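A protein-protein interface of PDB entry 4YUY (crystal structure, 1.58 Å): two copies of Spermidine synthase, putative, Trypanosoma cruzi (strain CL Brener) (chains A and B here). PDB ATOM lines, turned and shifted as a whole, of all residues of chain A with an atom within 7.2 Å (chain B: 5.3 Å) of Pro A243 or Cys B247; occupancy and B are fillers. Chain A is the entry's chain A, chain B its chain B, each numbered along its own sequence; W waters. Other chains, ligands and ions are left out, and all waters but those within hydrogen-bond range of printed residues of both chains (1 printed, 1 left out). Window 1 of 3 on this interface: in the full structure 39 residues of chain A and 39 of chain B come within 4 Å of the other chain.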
ATOM      1  N   MET A  32     -31.981 -22.029 -19.516  1.00  0.00           N
ATOM      2  CA  MET A  32     -32.010 -20.719 -20.072  1.00  0.00           C
ATOM      3  C   MET A  32     -33.141 -19.866 -19.412  1.00  0.00           C
ATOM      4  O   MET A  32     -34.270 -20.418 -19.133  1.00  0.00           O
ATOM      5  CB  MET A  32     -32.045 -20.764 -21.636  1.00  0.00           C
ATOM      6  CG  MET A  32     -32.086 -19.384 -22.298  1.00  0.00           C
ATOM      7  SD  MET A  32     -30.638 -18.463 -21.813  1.00  0.00           S
ATOM      8  CE  MET A  32     -30.775 -16.987 -22.775  1.00  0.00           C
ATOM      9  N   PRO A  60     -32.935  -7.701 -26.118  1.00  0.00           N
ATOM     10  CA  PRO A  60     -33.342  -7.643 -27.498  1.00  0.00           C
ATOM     11  C   PRO A  60     -34.448  -8.628 -27.911  1.00  0.00           C
ATOM     12  O   PRO A  60     -34.794  -8.640 -29.074  1.00  0.00           O
ATOM     13  CB  PRO A  60     -32.054  -8.105 -28.218  1.00  0.00           C
ATOM     14  CG  PRO A  60     -31.437  -9.091 -27.271  1.00  0.00           C
ATOM     15  CD  PRO A  60     -31.677  -8.455 -25.891  1.00  0.00           C
ATOM     16  N   TRP A  61     -34.924  -9.436 -26.961  1.00  0.00           N
ATOM     17  CA  TRP A  61     -35.682 -10.665 -27.366  1.00  0.00           C
ATOM     18  C   TRP A  61     -37.102 -10.408 -27.872  1.00  0.00           C
ATOM     19  O   TRP A  61     -37.672 -11.195 -28.663  1.00  0.00           O
ATOM     20  CB  TRP A  61     -35.655 -11.714 -26.242  1.00  0.00           C
ATOM     21  CG  TRP A  61     -34.208 -12.018 -25.935  1.00  0.00           C
ATOM     22  CD1 TRP A  61     -33.427 -11.495 -24.937  1.00  0.00           C
ATOM     23  CD2 TRP A  61     -33.334 -12.824 -26.763  1.00  0.00           C
ATOM     24  NE1 TRP A  61     -32.097 -11.984 -25.065  1.00  0.00           N
ATOM     25  CE2 TRP A  61     -32.041 -12.724 -26.230  1.00  0.00           C
ATOM     26  CE3 TRP A  61     -33.533 -13.541 -27.967  1.00  0.00           C
ATOM     27  CZ2 TRP A  61     -30.969 -13.352 -26.815  1.00  0.00           C
ATOM     28  CZ3 TRP A  61     -32.454 -14.186 -28.537  1.00  0.00           C
ATOM     29  CH2 TRP A  61     -31.193 -14.068 -27.962  1.00  0.00           C
ATOM     30  N   ILE A  71     -39.230 -22.838 -24.878  1.00  0.00           N
ATOM     31  CA  ILE A  71     -39.250 -21.660 -25.684  1.00  0.00           C
ATOM     32  C   ILE A  71     -39.306 -22.113 -27.135  1.00  0.00           C
ATOM     33  O   ILE A  71     -38.520 -22.997 -27.527  1.00  0.00           O
ATOM     34  CB  ILE A  71     -37.958 -20.817 -25.473  1.00  0.00           C
ATOM     35  CG1 ILE A  71     -37.999 -20.158 -24.114  1.00  0.00           C
ATOM     36  CG2 ILE A  71     -37.898 -19.739 -26.592  1.00  0.00           C
ATOM     37  CD1 ILE A  71     -36.634 -19.641 -23.616  1.00  0.00           C
ATOM     38  N   THR A  74     -38.818 -16.420 -30.438  1.00  0.00           N
ATOM     39  CA  THR A  74     -38.703 -15.050 -29.964  1.00  0.00           C
ATOM     40  C   THR A  74     -38.682 -14.175 -31.141  1.00  0.00           C
ATOM     41  O   THR A  74     -38.176 -14.573 -32.216  1.00  0.00           O
ATOM     42  CB  THR A  74     -37.444 -14.747 -29.088  1.00  0.00           C
ATOM     43  OG1 THR A  74     -36.270 -14.655 -29.933  1.00  0.00           O
ATOM     44  CG2 THR A  74     -37.233 -15.775 -28.011  1.00  0.00           C
ATOM     45  N   TYR A  76     -36.680 -11.900 -31.825  1.00  0.00           N
ATOM     46  CA  TYR A  76     -35.284 -11.578 -32.138  1.00  0.00           C
ATOM     47  C   TYR A  76     -34.565 -12.579 -32.964  1.00  0.00           C
ATOM     48  O   TYR A  76     -33.875 -12.199 -33.911  1.00  0.00           O
ATOM     49  CB  TYR A  76     -34.519 -11.298 -30.860  1.00  0.00           C
ATOM     50  CG  TYR A  76     -33.056 -10.767 -31.107  1.00  0.00           C
ATOM     51  CD1 TYR A  76     -32.862  -9.636 -31.884  1.00  0.00           C
ATOM     52  CD2 TYR A  76     -31.987 -11.303 -30.416  1.00  0.00           C
ATOM     53  CE1 TYR A  76     -31.573  -9.019 -32.027  1.00  0.00           C
ATOM     54  CE2 TYR A  76     -30.723 -10.740 -30.568  1.00  0.00           C
ATOM     55  CZ  TYR A  76     -30.524  -9.682 -31.413  1.00  0.00           C
ATOM     56  OH  TYR A  76     -29.259  -9.144 -31.503  1.00  0.00           O
ATOM     57  N   ASP A  77     -34.736 -13.867 -32.636  1.00  0.00           N
ATOM     58  CA  ASP A  77     -33.940 -14.857 -33.343  1.00  0.00           C
ATOM     59  C   ASP A  77     -34.808 -15.821 -34.210  1.00  0.00           C
ATOM     60  O   ASP A  77     -34.249 -16.821 -34.738  1.00  0.00           O
ATOM     61  CB  ASP A  77     -33.026 -15.672 -32.369  1.00  0.00           C
ATOM     62  CG  ASP A  77     -33.821 -16.531 -31.386  1.00  0.00           C
ATOM     63  OD1 ASP A  77     -35.116 -16.618 -31.505  1.00  0.00           O
ATOM     64  OD2 ASP A  77     -33.142 -17.208 -30.578  1.00  0.00           O
ATOM     65  N   VAL A  80     -33.762 -17.454 -37.810  1.00  0.00           N
ATOM     66  CA  VAL A  80     -32.690 -18.447 -38.092  1.00  0.00           C
ATOM     67  C   VAL A  80     -33.267 -19.823 -38.518  1.00  0.00           C
ATOM     68  O   VAL A  80     -33.078 -20.294 -39.640  1.00  0.00           O
ATOM     69  CB  VAL A  80     -31.764 -18.723 -36.875  1.00  0.00           C
ATOM     70  CG1 VAL A  80     -30.714 -19.808 -37.343  1.00  0.00           C
ATOM     71  CG2 VAL A  80     -31.008 -17.425 -36.461  1.00  0.00           C
ATOM     72  N   MET A 240     -27.349 -25.202 -36.848  1.00  0.00           N
ATOM     73  CA  MET A 240     -27.548 -23.784 -36.988  1.00  0.00           C
ATOM     74  C   MET A 240     -27.515 -23.112 -35.622  1.00  0.00           C
ATOM     75  O   MET A 240     -27.662 -23.758 -34.553  1.00  0.00           O
ATOM     76  CB  MET A 240     -28.887 -23.541 -37.614  1.00  0.00           C
ATOM     77  CG  MET A 240     -30.118 -23.873 -36.734  1.00  0.00           C
ATOM     78  SD  MET A 240     -31.697 -24.166 -37.712  1.00  0.00           S
ATOM     79  CE  MET A 240     -31.664 -25.941 -37.955  1.00  0.00           C
ATOM     80  N   HIS A 241     -27.321 -21.809 -35.661  1.00  0.00           N
ATOM     81  CA  HIS A 241     -27.116 -21.068 -34.403  1.00  0.00           C
ATOM     82  C   HIS A 241     -28.485 -20.471 -33.966  1.00  0.00           C
ATOM     83  O   HIS A 241     -28.927 -19.433 -34.516  1.00  0.00           O
ATOM     84  CB  HIS A 241     -26.062 -19.919 -34.648  1.00  0.00           C
ATOM     85  CG  HIS A 241     -24.638 -20.387 -34.827  1.00  0.00           C
ATOM     86  ND1 HIS A 241     -24.044 -20.567 -36.069  1.00  0.00           N
ATOM     87  CD2 HIS A 241     -23.672 -20.614 -33.914  1.00  0.00           C
ATOM     88  CE1 HIS A 241     -22.782 -20.928 -35.903  1.00  0.00           C
ATOM     89  NE2 HIS A 241     -22.552 -21.018 -34.606  1.00  0.00           N
ATOM     90  N   VAL A 242     -28.982 -20.933 -32.831  1.00  0.00           N
ATOM     91  CA  VAL A 242     -30.298 -20.455 -32.311  1.00  0.00           C
ATOM     92  C   VAL A 242     -30.172 -20.267 -30.828  1.00  0.00           C
ATOM     93  O   VAL A 242     -30.150 -21.227 -30.078  1.00  0.00           O
ATOM     94  CB  VAL A 242     -31.430 -21.469 -32.581  1.00  0.00           C
ATOM     95  CG1 VAL A 242     -32.745 -20.984 -31.948  1.00  0.00           C
ATOM     96  CG2 VAL A 242     -31.605 -21.691 -34.090  1.00  0.00           C
ATOM     97  N   PRO A 243     -29.956 -19.014 -30.413  1.00  0.00           N
ATOM     98  CA  PRO A 243     -29.673 -18.728 -28.954  1.00  0.00           C
ATOM     99  C   PRO A 243     -30.730 -19.244 -28.014  1.00  0.00           C
ATOM    100  O   PRO A 243     -30.331 -19.612 -26.878  1.00  0.00           O
ATOM    101  CB  PRO A 243     -29.767 -17.195 -28.951  1.00  0.00           C
ATOM    102  CG  PRO A 243     -29.221 -16.800 -30.317  1.00  0.00           C
ATOM    103  CD  PRO A 243     -29.843 -17.796 -31.216  1.00  0.00           C
ATOM    104  N   THR A 244     -31.980 -19.296 -28.467  1.00  0.00           N
ATOM    105  CA  THR A 244     -33.049 -19.627 -27.537  1.00  0.00           C
ATOM    106  C   THR A 244     -33.537 -21.094 -27.709  1.00  0.00           C
ATOM    107  O   THR A 244     -34.641 -21.444 -27.273  1.00  0.00           O
ATOM    108  CB  THR A 244     -34.220 -18.602 -27.566  1.00  0.00           C
ATOM    109  OG1 THR A 244     -34.681 -18.516 -28.859  1.00  0.00           O
ATOM    110  CG2 THR A 244     -33.724 -17.240 -27.151  1.00  0.00           C
ATOM    111  N   TYR A 245     -32.703 -21.971 -28.271  1.00  0.00           N
ATOM    112  CA  TYR A 245     -32.888 -23.384 -28.127  1.00  0.00           C
ATOM    113  C   TYR A 245     -31.812 -23.886 -27.174  1.00  0.00           C
ATOM    114  O   TYR A 245     -30.678 -23.376 -27.184  1.00  0.00           O
ATOM    115  CB  TYR A 245     -32.818 -24.131 -29.505  1.00  0.00           C
ATOM    116  CG  TYR A 245     -33.103 -25.622 -29.354  1.00  0.00           C
ATOM    117  CD1 TYR A 245     -32.080 -26.556 -29.005  1.00  0.00           C
ATOM    118  CD2 TYR A 245     -34.425 -26.070 -29.491  1.00  0.00           C
ATOM    119  CE1 TYR A 245     -32.363 -27.879 -28.827  1.00  0.00           C
ATOM    120  CE2 TYR A 245     -34.756 -27.414 -29.289  1.00  0.00           C
ATOM    121  CZ  TYR A 245     -33.740 -28.301 -28.977  1.00  0.00           C
ATOM    122  OH  TYR A 245     -34.094 -29.605 -28.816  1.00  0.00           O
ATOM    123  N   PRO A 246     -32.122 -24.910 -26.340  1.00  0.00           N
ATOM    124  CA  PRO A 246     -31.152 -25.343 -25.324  1.00  0.00           C
ATOM    125  C   PRO A 246     -29.754 -25.654 -25.866  1.00  0.00           C
ATOM    126  O   PRO A 246     -29.661 -26.391 -26.877  1.00  0.00           O
ATOM    127  CB  PRO A 246     -31.870 -26.572 -24.702  1.00  0.00           C
ATOM    128  CG  PRO A 246     -33.289 -26.122 -24.751  1.00  0.00           C
ATOM    129  CD  PRO A 246     -33.441 -25.530 -26.149  1.00  0.00           C
ATOM    130  N   CYS A 247     -28.729 -24.996 -25.259  1.00  0.00           N
ATOM    131  CA  CYS A 247     -27.282 -25.096 -25.615  1.00  0.00           C
ATOM    132  C   CYS A 247     -26.905 -24.283 -26.841  1.00  0.00           C
ATOM    133  O   CYS A 247     -25.731 -24.330 -27.256  1.00  0.00           O
ATOM    134  CB  CYS A 247     -26.761 -26.526 -25.819  1.00  0.00           C
ATOM    135  SG  CYS A 247     -26.781 -27.509 -24.308  1.00  0.00           S
ATOM    136  N   GLY A 248     -27.883 -23.583 -27.415  1.00  0.00           N
ATOM    137  CA  GLY A 248     -27.564 -22.528 -28.445  1.00  0.00           C
ATOM    138  C   GLY A 248     -27.530 -23.036 -29.859  1.00  0.00           C
ATOM    139  O   GLY A 248     -27.150 -22.269 -30.739  1.00  0.00           O
ATOM    140  N   SER A 249     -27.945 -24.271 -30.139  1.00  0.00           N
ATOM    141  CA  SER A 249     -28.010 -24.674 -31.518  1.00  0.00           C
ATOM    142  C   SER A 249     -29.065 -25.744 -31.661  1.00  0.00           C
ATOM    143  O   SER A 249     -29.624 -26.260 -30.671  1.00  0.00           O
ATOM    144  CB  SER A 249     -26.704 -25.229 -31.930  1.00  0.00           C
ATOM    145  OG  SER A 249     -26.357 -26.440 -31.215  1.00  0.00           O
ATOM    146  N   GLN B  30     -31.453 -11.580 -19.966  1.00  0.00           N
ATOM    147  CA  GLN B  30     -31.188 -12.996 -20.176  1.00  0.00           C
ATOM    148  C   GLN B  30     -30.180 -13.524 -19.190  1.00  0.00           C
ATOM    149  O   GLN B  30     -29.317 -12.784 -18.721  1.00  0.00           O
ATOM    150  CB  GLN B  30     -30.711 -13.295 -21.580  1.00  0.00           C
ATOM    151  CG  GLN B  30     -29.252 -12.964 -21.862  1.00  0.00           C
ATOM    152  CD  GLN B  30     -28.950 -13.013 -23.335  1.00  0.00           C
ATOM    153  OE1 GLN B  30     -28.237 -13.959 -23.739  1.00  0.00           O
ATOM    154  NE2 GLN B  30     -29.363 -12.057 -24.095  1.00  0.00           N
ATOM    155  N   SER B 212     -19.966 -12.107 -28.961  1.00  0.00           N
ATOM    156  CA  SER B 212     -21.164 -12.685 -29.584  1.00  0.00           C
ATOM    157  C   SER B 212     -21.730 -11.824 -30.683  1.00  0.00           C
ATOM    158  O   SER B 212     -22.004 -10.603 -30.409  1.00  0.00           O
ATOM    159  CB  SER B 212     -22.276 -12.791 -28.513  1.00  0.00           C
ATOM    160  OG  SER B 212     -23.532 -13.173 -29.119  1.00  0.00           O
ATOM    161  N   TRP B 214     -24.666 -11.801 -31.462  1.00  0.00           N
ATOM    162  CA  TRP B 214     -26.071 -11.575 -31.068  1.00  0.00           C
ATOM    163  C   TRP B 214     -26.090 -10.453 -30.103  1.00  0.00           C
ATOM    164  O   TRP B 214     -27.175  -9.852 -29.883  1.00  0.00           O
ATOM    165  CB  TRP B 214     -26.597 -12.830 -30.349  1.00  0.00           C
ATOM    166  CG  TRP B 214     -26.753 -13.965 -31.279  1.00  0.00           C
ATOM    167  CD1 TRP B 214     -25.964 -15.129 -31.353  1.00  0.00           C
ATOM    168  CD2 TRP B 214     -27.776 -14.108 -32.276  1.00  0.00           C
ATOM    169  NE1 TRP B 214     -26.442 -15.932 -32.379  1.00  0.00           N
ATOM    170  CE2 TRP B 214     -27.539 -15.344 -32.948  1.00  0.00           C
ATOM    171  CE3 TRP B 214     -28.870 -13.312 -32.662  1.00  0.00           C
ATOM    172  CZ2 TRP B 214     -28.404 -15.824 -33.988  1.00  0.00           C
ATOM    173  CZ3 TRP B 214     -29.742 -13.770 -33.679  1.00  0.00           C
ATOM    174  CH2 TRP B 214     -29.459 -15.019 -34.355  1.00  0.00           C
ATOM    175  N   LEU B 215     -24.963 -10.181 -29.432  1.00  0.00           N
ATOM    176  CA  LEU B 215     -24.981  -9.195 -28.270  1.00  0.00           C
ATOM    177  C   LEU B 215     -24.024  -8.014 -28.446  1.00  0.00           C
ATOM    178  O   LEU B 215     -24.256  -6.921 -27.915  1.00  0.00           O
ATOM    179  CB  LEU B 215     -24.608  -9.882 -26.945  1.00  0.00           C
ATOM    180  CG  LEU B 215     -25.581 -11.027 -26.615  1.00  0.00           C
ATOM    181  CD1 LEU B 215     -24.969 -11.957 -25.585  1.00  0.00           C
ATOM    182  CD2 LEU B 215     -26.966 -10.549 -26.163  1.00  0.00           C
ATOM    183  N   TYR B 245     -21.221 -19.935 -23.518  1.00  0.00           N
ATOM    184  CA  TYR B 245     -21.067 -18.505 -23.682  1.00  0.00           C
ATOM    185  C   TYR B 245     -22.452 -17.921 -24.022  1.00  0.00           C
ATOM    186  O   TYR B 245     -23.212 -18.564 -24.700  1.00  0.00           O
ATOM    187  CB  TYR B 245     -20.063 -18.208 -24.860  1.00  0.00           C
ATOM    188  CG  TYR B 245     -19.733 -16.727 -24.951  1.00  0.00           C
ATOM    189  CD1 TYR B 245     -18.770 -16.189 -24.079  1.00  0.00           C
ATOM    190  CD2 TYR B 245     -20.355 -15.851 -25.900  1.00  0.00           C
ATOM    191  CE1 TYR B 245     -18.445 -14.843 -24.077  1.00  0.00           C
ATOM    192  CE2 TYR B 245     -20.051 -14.483 -25.908  1.00  0.00           C
ATOM    193  CZ  TYR B 245     -19.055 -13.994 -24.988  1.00  0.00           C
ATOM    194  OH  TYR B 245     -18.723 -12.642 -24.955  1.00  0.00           O
ATOM    195  N   PRO B 246     -22.789 -16.671 -23.571  1.00  0.00           N
ATOM    196  CA  PRO B 246     -24.131 -16.077 -23.753  1.00  0.00           C
ATOM    197  C   PRO B 246     -24.568 -16.119 -25.231  1.00  0.00           C
ATOM    198  O   PRO B 246     -23.817 -15.667 -26.155  1.00  0.00           O
ATOM    199  CB  PRO B 246     -23.968 -14.686 -23.164  1.00  0.00           C
ATOM    200  CG  PRO B 246     -22.953 -14.896 -21.997  1.00  0.00           C
ATOM    201  CD  PRO B 246     -21.949 -15.893 -22.630  1.00  0.00           C
ATOM    202  N   CYS B 247     -25.743 -16.720 -25.428  1.00  0.00           N
ATOM    203  CA  CYS B 247     -26.337 -16.923 -26.761  1.00  0.00           C
ATOM    204  C   CYS B 247     -25.815 -18.149 -27.537  1.00  0.00           C
ATOM    205  O   CYS B 247     -26.372 -18.397 -28.620  1.00  0.00           O
ATOM    206  CB  CYS B 247     -26.324 -15.663 -27.647  1.00  0.00           C
ATOM    207  SG  CYS B 247     -27.376 -14.341 -26.959  1.00  0.00           S
ATOM    208  N   GLY B 248     -24.769 -18.845 -27.003  1.00  0.00           N
ATOM    209  CA  GLY B 248     -24.314 -20.127 -27.566  1.00  0.00           C
ATOM    210  C   GLY B 248     -23.331 -20.082 -28.674  1.00  0.00           C
ATOM    211  O   GLY B 248     -22.994 -21.133 -29.193  1.00  0.00           O
ATOM    212  N   SER B 249     -22.875 -18.897 -29.009  1.00  0.00           N
ATOM    213  CA  SER B 249     -21.701 -18.874 -29.874  1.00  0.00           C
ATOM    214  C   SER B 249     -20.711 -17.853 -29.493  1.00  0.00           C
ATOM    215  O   SER B 249     -21.087 -16.814 -28.967  1.00  0.00           O
ATOM    216  CB  SER B 249     -22.126 -18.680 -31.263  1.00  0.00           C
ATOM    217  OG  SER B 249     -22.711 -17.397 -31.486  1.00  0.00           O
HETATM  218  O   HOH W   1     -24.609 -21.385 -31.431  1.00  0.00           O
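CE of Met A32 touches CB of Gln B30, 3.9 Å away. Trp A61 touches Cys B247. Val A80 touches Trp B214. O of His A241 touches CZ2 of Trp B214 (3.7 Å). His A241 touches Ser B249. Pro A243 touches Trp B214 (CG to CE2, 3.4 Å). Pro A243 touches Cys B247.
Water W1 lies within hydrogen-bond range of the backbone carbonyl oxygen of Gly B248 (2.8 Å) and the backbone carbonyl oxygen of Gly A248 (2.8 Å).
Positions printed for both chains: 245, 246, 247, 248 and 249. Of the 9 pairs that touch across the chains among the printed residues, none has its exchanged pair printed and touching as well.
The backbone carbonyl oxygen of Trp A61 lies within hydrogen-bond range of the backbone NH of Tyr A76, 3.4 Å away. N of Tyr A76 sits close to OG1 of Thr A74 (3.4 Å). The side-chain amide oxygen of Gln B30 lies within hydrogen-bond range of the side-chain sulfur of Cys B247, at 3.4 Å. The side-chain hydroxyl (OG) of Ser B212 is in hydrogen-bond range of the backbone NH (N) of Trp B214.
Of chain B, only Trp B214 and Cys B247 come within 4 Å of Pro A243. Cys B247 touches two residues of chain A. Printed residues of chain A within 4 Å of Gln B30: Met A32 (3.9 Å) and Trp A61 (2.9 Å). Printed residues of chain B within 4 Å of Trp A61: Gln B30 and Cys B247. Printed residues of chain A within 4 Å of Trp B214: Tyr A76 (2.7 Å), Val A80 (3.6 Å), His A241 (3.7 Å) and Pro A243 (3.4 Å). Val A242 touches none of the printed residues of chain B. Gly A248 touches none of the printed residues of chain B. The nearest printed residue of chain B that does not touch Pro A243 is Gly B248 (5.3 Å). The nearest residue of chain A that does not touch Cys B247 is Gly A248 (4.3 Å).
The indole nitrogen of Trp A61 lies close to the side-chain amide nitrogen of Gln B30. O of Trp B214 lies within hydrogen-bond range of OH of Tyr A76, at 2.7 Å.
Along chain A the printed residues that touch a printed residue of chain B span positions 32 to 243. Printed residues of chain B that touch a printed residue of chain A: Gln B30, Trp B214, Cys B247 and Ser B249.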
